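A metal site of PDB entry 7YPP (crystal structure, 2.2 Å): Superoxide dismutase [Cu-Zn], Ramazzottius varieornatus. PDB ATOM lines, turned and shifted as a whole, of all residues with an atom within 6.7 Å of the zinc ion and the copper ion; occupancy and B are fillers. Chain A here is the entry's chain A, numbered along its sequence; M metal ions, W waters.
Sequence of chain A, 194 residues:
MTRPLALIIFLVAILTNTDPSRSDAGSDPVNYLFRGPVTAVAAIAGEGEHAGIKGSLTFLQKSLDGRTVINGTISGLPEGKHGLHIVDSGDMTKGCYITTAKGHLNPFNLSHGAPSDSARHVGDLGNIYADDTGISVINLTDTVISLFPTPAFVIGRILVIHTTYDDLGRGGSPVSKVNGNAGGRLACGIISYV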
ATOM      1  N   GLY A  83     -29.540 -31.190  -2.828  1.00  0.00           N
ATOM      2  CA  GLY A  83     -28.340 -31.021  -2.037  1.00  0.00           C
ATOM      3  C   GLY A  83     -28.071 -32.271  -1.187  1.00  0.00           C
ATOM      4  O   GLY A  83     -28.983 -32.820  -0.558  1.00  0.00           O
ATOM      5  N   LEU A  84     -26.807 -32.691  -1.176  1.00  0.00           N
ATOM      6  CA  LEU A  84     -26.362 -33.821  -0.382  1.00  0.00           C
ATOM      7  C   LEU A  84     -25.305 -33.322   0.602  1.00  0.00           C
ATOM      8  O   LEU A  84     -24.209 -32.955   0.194  1.00  0.00           O
ATOM      9  CB  LEU A  84     -25.799 -34.875  -1.333  1.00  0.00           C
ATOM     10  CG  LEU A  84     -25.355 -36.191  -0.697  1.00  0.00           C
ATOM     11  CD1 LEU A  84     -26.561 -37.003  -0.214  1.00  0.00           C
ATOM     12  CD2 LEU A  84     -24.491 -36.971  -1.676  1.00  0.00           C
ATOM     13  N   HIS A  85     -25.639 -33.274   1.885  1.00  0.00           N
ATOM     14  CA  HIS A  85     -24.764 -32.631   2.846  1.00  0.00           C
ATOM     15  C   HIS A  85     -24.632 -33.474   4.110  1.00  0.00           C
ATOM     16  O   HIS A  85     -25.561 -34.177   4.497  1.00  0.00           O
ATOM     17  CB  HIS A  85     -25.277 -31.246   3.238  1.00  0.00           C
ATOM     18  CG  HIS A  85     -25.488 -30.309   2.092  1.00  0.00           C
ATOM     19  ND1 HIS A  85     -26.545 -29.396   2.089  1.00  0.00           N
ATOM     20  CD2 HIS A  85     -24.834 -30.129   0.922  1.00  0.00           C
ATOM     21  CE1 HIS A  85     -26.496 -28.687   0.986  1.00  0.00           C
ATOM     22  NE2 HIS A  85     -25.456 -29.107   0.255  1.00  0.00           N
ATOM     23  N   ILE A  86     -23.456 -33.377   4.753  1.00  0.00           N
ATOM     24  CA  ILE A  86     -23.235 -33.986   6.043  1.00  0.00           C
ATOM     25  C   ILE A  86     -23.335 -32.876   7.086  1.00  0.00           C
ATOM     26  O   ILE A  86     -22.630 -31.880   6.961  1.00  0.00           O
ATOM     27  CB  ILE A  86     -21.886 -34.742   6.083  1.00  0.00           C
ATOM     28  CG1 ILE A  86     -21.769 -35.751   4.928  1.00  0.00           C
ATOM     29  CG2 ILE A  86     -21.673 -35.416   7.430  1.00  0.00           C
ATOM     30  CD1 ILE A  86     -20.394 -36.375   4.788  1.00  0.00           C
ATOM     31  N   VAL A  87     -24.210 -33.031   8.090  1.00  0.00           N
ATOM     32  CA  VAL A  87     -24.409 -32.004   9.113  1.00  0.00           C
ATOM     33  C   VAL A  87     -23.542 -32.311  10.334  1.00  0.00           C
ATOM     34  O   VAL A  87     -22.949 -33.389  10.411  1.00  0.00           O
ATOM     35  CB  VAL A  87     -25.900 -31.798   9.482  1.00  0.00           C
ATOM     36  CG1 VAL A  87     -26.679 -31.199   8.336  1.00  0.00           C
ATOM     37  CG2 VAL A  87     -26.549 -33.089   9.964  1.00  0.00           C
ATOM     38  N   HIS A 104     -23.814 -27.446   8.581  1.00  0.00           N
ATOM     39  CA  HIS A 104     -23.013 -28.444   7.897  1.00  0.00           C
ATOM     40  C   HIS A 104     -21.759 -28.788   8.713  1.00  0.00           C
ATOM     41  O   HIS A 104     -21.214 -27.916   9.378  1.00  0.00           O
ATOM     42  CB  HIS A 104     -22.631 -27.965   6.492  1.00  0.00           C
ATOM     43  CG  HIS A 104     -23.797 -27.813   5.588  1.00  0.00           C
ATOM     44  ND1 HIS A 104     -23.687 -27.222   4.345  1.00  0.00           N
ATOM     45  CD2 HIS A 104     -25.108 -28.134   5.766  1.00  0.00           C
ATOM     46  CE1 HIS A 104     -24.870 -27.213   3.766  1.00  0.00           C
ATOM     47  NE2 HIS A 104     -25.765 -27.751   4.614  1.00  0.00           N
ATOM     48  N   LEU A 105     -21.298 -30.035   8.604  1.00  0.00           N
ATOM     49  CA  LEU A 105     -20.044 -30.446   9.233  1.00  0.00           C
ATOM     50  C   LEU A 105     -18.908 -29.550   8.737  1.00  0.00           C
ATOM     51  O   LEU A 105     -18.595 -29.554   7.552  1.00  0.00           O
ATOM     52  CB  LEU A 105     -19.796 -31.925   8.925  1.00  0.00           C
ATOM     53  CG  LEU A 105     -18.566 -32.536   9.615  1.00  0.00           C
ATOM     54  CD1 LEU A 105     -18.696 -32.468  11.130  1.00  0.00           C
ATOM     55  CD2 LEU A 105     -18.267 -33.948   9.139  1.00  0.00           C
ATOM     56  N   SER A 111     -16.474 -21.337   4.631  1.00  0.00           N
ATOM     57  CA  SER A 111     -17.808 -21.037   4.146  1.00  0.00           C
ATOM     58  C   SER A 111     -18.307 -22.190   3.249  1.00  0.00           C
ATOM     59  O   SER A 111     -17.540 -23.056   2.872  1.00  0.00           O
ATOM     60  CB  SER A 111     -17.856 -19.703   3.435  1.00  0.00           C
ATOM     61  OG  SER A 111     -16.895 -19.692   2.394  1.00  0.00           O
ATOM     62  N   HIS A 112     -19.602 -22.183   2.942  1.00  0.00           N
ATOM     63  CA  HIS A 112     -20.227 -23.204   2.122  1.00  0.00           C
ATOM     64  C   HIS A 112     -19.781 -23.039   0.665  1.00  0.00           C
ATOM     65  O   HIS A 112     -19.720 -21.924   0.141  1.00  0.00           O
ATOM     66  CB  HIS A 112     -21.753 -23.136   2.222  1.00  0.00           C
ATOM     67  CG  HIS A 112     -22.441 -24.152   1.377  1.00  0.00           C
ATOM     68  ND1 HIS A 112     -22.605 -25.452   1.786  1.00  0.00           N
ATOM     69  CD2 HIS A 112     -22.959 -24.080   0.129  1.00  0.00           C
ATOM     70  CE1 HIS A 112     -23.209 -26.144   0.836  1.00  0.00           C
ATOM     71  NE2 HIS A 112     -23.440 -25.327  -0.192  1.00  0.00           N
ATOM     72  N   GLY A 113     -19.481 -24.179   0.003  1.00  0.00           N
ATOM     73  CA  GLY A 113     -19.190 -24.157  -1.427  1.00  0.00           C
ATOM     74  C   GLY A 113     -19.533 -25.482  -2.092  1.00  0.00           C
ATOM     75  O   GLY A 113     -20.087 -26.373  -1.457  1.00  0.00           O
ATOM     76  N   ARG A 120     -15.010 -24.648   1.319  1.00  0.00           N
ATOM     77  CA  ARG A 120     -16.163 -25.533   1.456  1.00  0.00           C
ATOM     78  C   ARG A 120     -16.164 -26.142   2.846  1.00  0.00           C
ATOM     79  O   ARG A 120     -15.142 -26.134   3.522  1.00  0.00           O
ATOM     80  CB  ARG A 120     -16.140 -26.668   0.420  1.00  0.00           C
ATOM     81  CG  ARG A 120     -14.891 -27.536   0.485  1.00  0.00           C
ATOM     82  CD  ARG A 120     -15.068 -28.842  -0.258  1.00  0.00           C
ATOM     83  NE  ARG A 120     -15.732 -29.855   0.538  1.00  0.00           N
ATOM     84  CZ  ARG A 120     -15.809 -31.139   0.211  1.00  0.00           C
ATOM     85  NH1 ARG A 120     -15.270 -31.566  -0.930  1.00  0.00           N
ATOM     86  NH2 ARG A 120     -16.404 -31.988   1.032  1.00  0.00           N
ATOM     87  N   HIS A 121     -17.332 -26.630   3.269  1.00  0.00           N
ATOM     88  CA  HIS A 121     -17.470 -27.441   4.468  1.00  0.00           C
ATOM     89  C   HIS A 121     -17.035 -28.868   4.169  1.00  0.00           C
ATOM     90  O   HIS A 121     -17.127 -29.294   3.019  1.00  0.00           O
ATOM     91  CB  HIS A 121     -18.916 -27.435   4.943  1.00  0.00           C
ATOM     92  CG  HIS A 121     -19.461 -26.073   5.201  1.00  0.00           C
ATOM     93  ND1 HIS A 121     -20.729 -25.697   4.797  1.00  0.00           N
ATOM     94  CD2 HIS A 121     -18.920 -24.992   5.818  1.00  0.00           C
ATOM     95  CE1 HIS A 121     -20.950 -24.461   5.164  1.00  0.00           C
ATOM     96  NE2 HIS A 121     -19.862 -24.001   5.792  1.00  0.00           N
ATOM     97  N   VAL A 122     -16.572 -29.590   5.201  1.00  0.00           N
ATOM     98  CA  VAL A 122     -16.302 -31.011   5.031  1.00  0.00           C
ATOM     99  C   VAL A 122     -17.558 -31.670   4.477  1.00  0.00           C
ATOM    100  O   VAL A 122     -17.476 -32.525   3.600  1.00  0.00           O
ATOM    101  CB  VAL A 122     -15.816 -31.664   6.337  1.00  0.00           C
ATOM    102  CG1 VAL A 122     -15.857 -33.194   6.241  1.00  0.00           C
ATOM    103  CG2 VAL A 122     -14.408 -31.243   6.692  1.00  0.00           C
ATOM    104  N   GLY A 123     -18.728 -31.223   4.969  1.00  0.00           N
ATOM    105  CA  GLY A 123     -20.001 -31.870   4.692  1.00  0.00           C
ATOM    106  C   GLY A 123     -20.607 -31.518   3.328  1.00  0.00           C
ATOM    107  O   GLY A 123     -21.727 -31.956   3.033  1.00  0.00           O
ATOM    108  N   ASP A 124     -19.882 -30.749   2.503  1.00  0.00           N
ATOM    109  CA  ASP A 124     -20.426 -30.246   1.257  1.00  0.00           C
ATOM    110  C   ASP A 124     -20.165 -31.243   0.129  1.00  0.00           C
ATOM    111  O   ASP A 124     -19.099 -31.186  -0.518  1.00  0.00           O
ATOM    112  CB  ASP A 124     -19.836 -28.873   0.904  1.00  0.00           C
ATOM    113  CG  ASP A 124     -20.269 -27.767   1.863  1.00  0.00           C
ATOM    114  OD1 ASP A 124     -21.191 -28.018   2.660  1.00  0.00           O
ATOM    115  OD2 ASP A 124     -19.672 -26.658   1.799  1.00  0.00           O
ATOM    116  N   VAL A 160     -27.710 -35.746   4.763  1.00  0.00           N
ATOM    117  CA  VAL A 160     -29.027 -35.182   4.494  1.00  0.00           C
ATOM    118  C   VAL A 160     -29.229 -35.090   2.984  1.00  0.00           C
ATOM    119  O   VAL A 160     -28.305 -34.709   2.266  1.00  0.00           O
ATOM    120  CB  VAL A 160     -29.158 -33.804   5.174  1.00  0.00           C
ATOM    121  CG1 VAL A 160     -30.298 -33.005   4.598  1.00  0.00           C
ATOM    122  CG2 VAL A 160     -29.319 -33.921   6.686  1.00  0.00           C
ATOM    123  N   HIS A 162     -31.599 -32.883   0.597  1.00  0.00           N
ATOM    124  CA  HIS A 162     -32.392 -31.665   0.748  1.00  0.00           C
ATOM    125  C   HIS A 162     -33.584 -31.643  -0.213  1.00  0.00           C
ATOM    126  O   HIS A 162     -33.591 -32.326  -1.247  1.00  0.00           O
ATOM    127  CB  HIS A 162     -31.505 -30.427   0.559  1.00  0.00           C
ATOM    128  CG  HIS A 162     -30.765 -30.047   1.791  1.00  0.00           C
ATOM    129  ND1 HIS A 162     -31.346 -29.356   2.830  1.00  0.00           N
ATOM    130  CD2 HIS A 162     -29.494 -30.254   2.158  1.00  0.00           C
ATOM    131  CE1 HIS A 162     -30.460 -29.151   3.791  1.00  0.00           C
ATOM    132  NE2 HIS A 162     -29.328 -29.697   3.402  1.00  0.00           N
ATOM    133  N   ASP A 166     -28.571 -27.504  -4.110  1.00  0.00           N
ATOM    134  CA  ASP A 166     -27.569 -26.669  -3.487  1.00  0.00           C
ATOM    135  C   ASP A 166     -27.084 -25.663  -4.526  1.00  0.00           C
ATOM    136  O   ASP A 166     -26.731 -26.075  -5.631  1.00  0.00           O
ATOM    137  CB  ASP A 166     -26.427 -27.582  -3.009  1.00  0.00           C
ATOM    138  CG  ASP A 166     -25.261 -26.895  -2.317  1.00  0.00           C
ATOM    139  OD1 ASP A 166     -25.190 -25.640  -2.299  1.00  0.00           O
ATOM    140  OD2 ASP A 166     -24.403 -27.646  -1.796  1.00  0.00           O
ATOM    141  N   LYS A 177     -23.926 -18.835   1.335  1.00  0.00           N
ATOM    142  CA  LYS A 177     -22.585 -19.089   1.836  1.00  0.00           C
ATOM    143  C   LYS A 177     -22.670 -19.828   3.169  1.00  0.00           C
ATOM    144  O   LYS A 177     -21.643 -20.196   3.760  1.00  0.00           O
ATOM    145  CB  LYS A 177     -21.805 -17.767   1.960  1.00  0.00           C
ATOM    146  CG  LYS A 177     -21.443 -17.076   0.646  1.00  0.00           C
ATOM    147  CD  LYS A 177     -20.421 -17.836  -0.167  1.00  0.00           C
ATOM    148  CE  LYS A 177     -19.824 -17.006  -1.292  1.00  0.00           C
ATOM    149  NZ  LYS A 177     -19.402 -17.864  -2.423  1.00  0.00           N
ATOM    150  N   VAL A 178     -23.897 -20.054   3.644  1.00  0.00           N
ATOM    151  CA  VAL A 178     -24.107 -20.814   4.863  1.00  0.00           C
ATOM    152  C   VAL A 178     -24.421 -22.270   4.520  1.00  0.00           C
ATOM    153  O   VAL A 178     -23.771 -23.180   5.049  1.00  0.00           O
ATOM    154  CB  VAL A 178     -25.177 -20.173   5.778  1.00  0.00           C
ATOM    155  CG1 VAL A 178     -25.480 -21.002   7.025  1.00  0.00           C
ATOM    156  CG2 VAL A 178     -24.760 -18.757   6.195  1.00  0.00           C
ATOM    157  N   ASN A 179     -25.369 -22.523   3.609  1.00  0.00           N
ATOM    158  CA  ASN A 179     -25.791 -23.891   3.385  1.00  0.00           C
ATOM    159  C   ASN A 179     -26.244 -24.143   1.948  1.00  0.00           C
ATOM    160  O   ASN A 179     -26.736 -25.230   1.659  1.00  0.00           O
ATOM    161  CB  ASN A 179     -26.891 -24.320   4.359  1.00  0.00           C
ATOM    162  CG  ASN A 179     -28.072 -23.376   4.345  1.00  0.00           C
ATOM    163  OD1 ASN A 179     -28.553 -22.981   3.273  1.00  0.00           O
ATOM    164  ND2 ASN A 179     -28.503 -22.969   5.524  1.00  0.00           N
ATOM    165  N   GLY A 180     -26.089 -23.157   1.058  1.00  0.00           N
ATOM    166  CA  GLY A 180     -26.396 -23.342  -0.346  1.00  0.00           C
ATOM    167  C   GLY A 180     -27.885 -23.220  -0.675  1.00  0.00           C
ATOM    168  O   GLY A 180     -28.294 -23.551  -1.785  1.00  0.00           O
ATOM    169  N   ALA A 182     -30.615 -24.892   0.073  1.00  0.00           N
ATOM    170  CA  ALA A 182     -31.126 -26.118  -0.513  1.00  0.00           C
ATOM    171  C   ALA A 182     -32.455 -26.501   0.119  1.00  0.00           C
ATOM    172  O   ALA A 182     -33.035 -27.532  -0.217  1.00  0.00           O
ATOM    173  CB  ALA A 182     -30.093 -27.219  -0.408  1.00  0.00           C
ATOM    174  N   GLY A 183     -32.942 -25.642   1.034  1.00  0.00           N
ATOM    175  CA  GLY A 183     -34.249 -25.826   1.636  1.00  0.00           C
ATOM    176  C   GLY A 183     -34.218 -26.849   2.769  1.00  0.00           C
ATOM    177  O   GLY A 183     -33.179 -27.094   3.389  1.00  0.00           O
HETATM  178 ZN    ZN M   1     -21.925 -26.462   3.478  1.00  0.00          ZN
HETATM  179 CU    CU M   2     -27.368 -28.713   3.719  1.00  0.00          CU
HETATM  180  O   HOH W   1     -28.796 -26.307   2.516  1.00  0.00           O
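A ring nitrogen (NE2) of His 112 is in hydrogen-bond range of the side-chain carboxylate (OD1) of Asp 166, at 2.8 Å. The backbone NH (N) of His 112 lies within hydrogen-bond range of the backbone carbonyl oxygen (O) of Lys 177 (3.0 Å). The backbone carbonyl oxygen (O) of His 85 sits at hydrogen-bond distance from the backbone NH (N) of Val 160, at 2.7 Å. A ring nitrogen (ND1) of His 162 lies within hydrogen-bond range of the backbone carbonyl oxygen (O) of Gly 183, at 3.0 Å. NH2 of Arg 120 sits at hydrogen-bond distance from O of Asp 124 (3.2 Å). O of Gly 83 sits at hydrogen-bond distance from N of His 162, 2.9 Å away. The backbone NH (N) of Gly 113 is in hydrogen-bond range of the side-chain carboxylate (OD2) of Asp 124. A ring nitrogen (NE2) of His 85 lies within hydrogen-bond range of the side-chain carboxylate (OD2) of Asp 166 (2.7 Å).
Within 4 Å of the zinc ion: His 104, His 112, His 121 and Asp 124.
Within 4 Å of the copper ion: His 85, His 104 and His 162. The nearest printed residue that does not touch the copper ion is Asn 179 (4.1 Å).
The zinc ion is bound by OD1 of Asp 124 (1.9 Å), ND1 of His 121 (1.9 Å), ND1 of His 112 (2.1 Å) and ND1 of His 104 (2.1 Å). Slightly farther from the zinc ion lies the side-chain carboxylate (OD2) of Asp 124 (2.8 Å).
The copper ion is bound by ND1 of His 85, NE2 of His 104 and NE2 of His 162. The copper ion has three donor atoms within binding distance.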
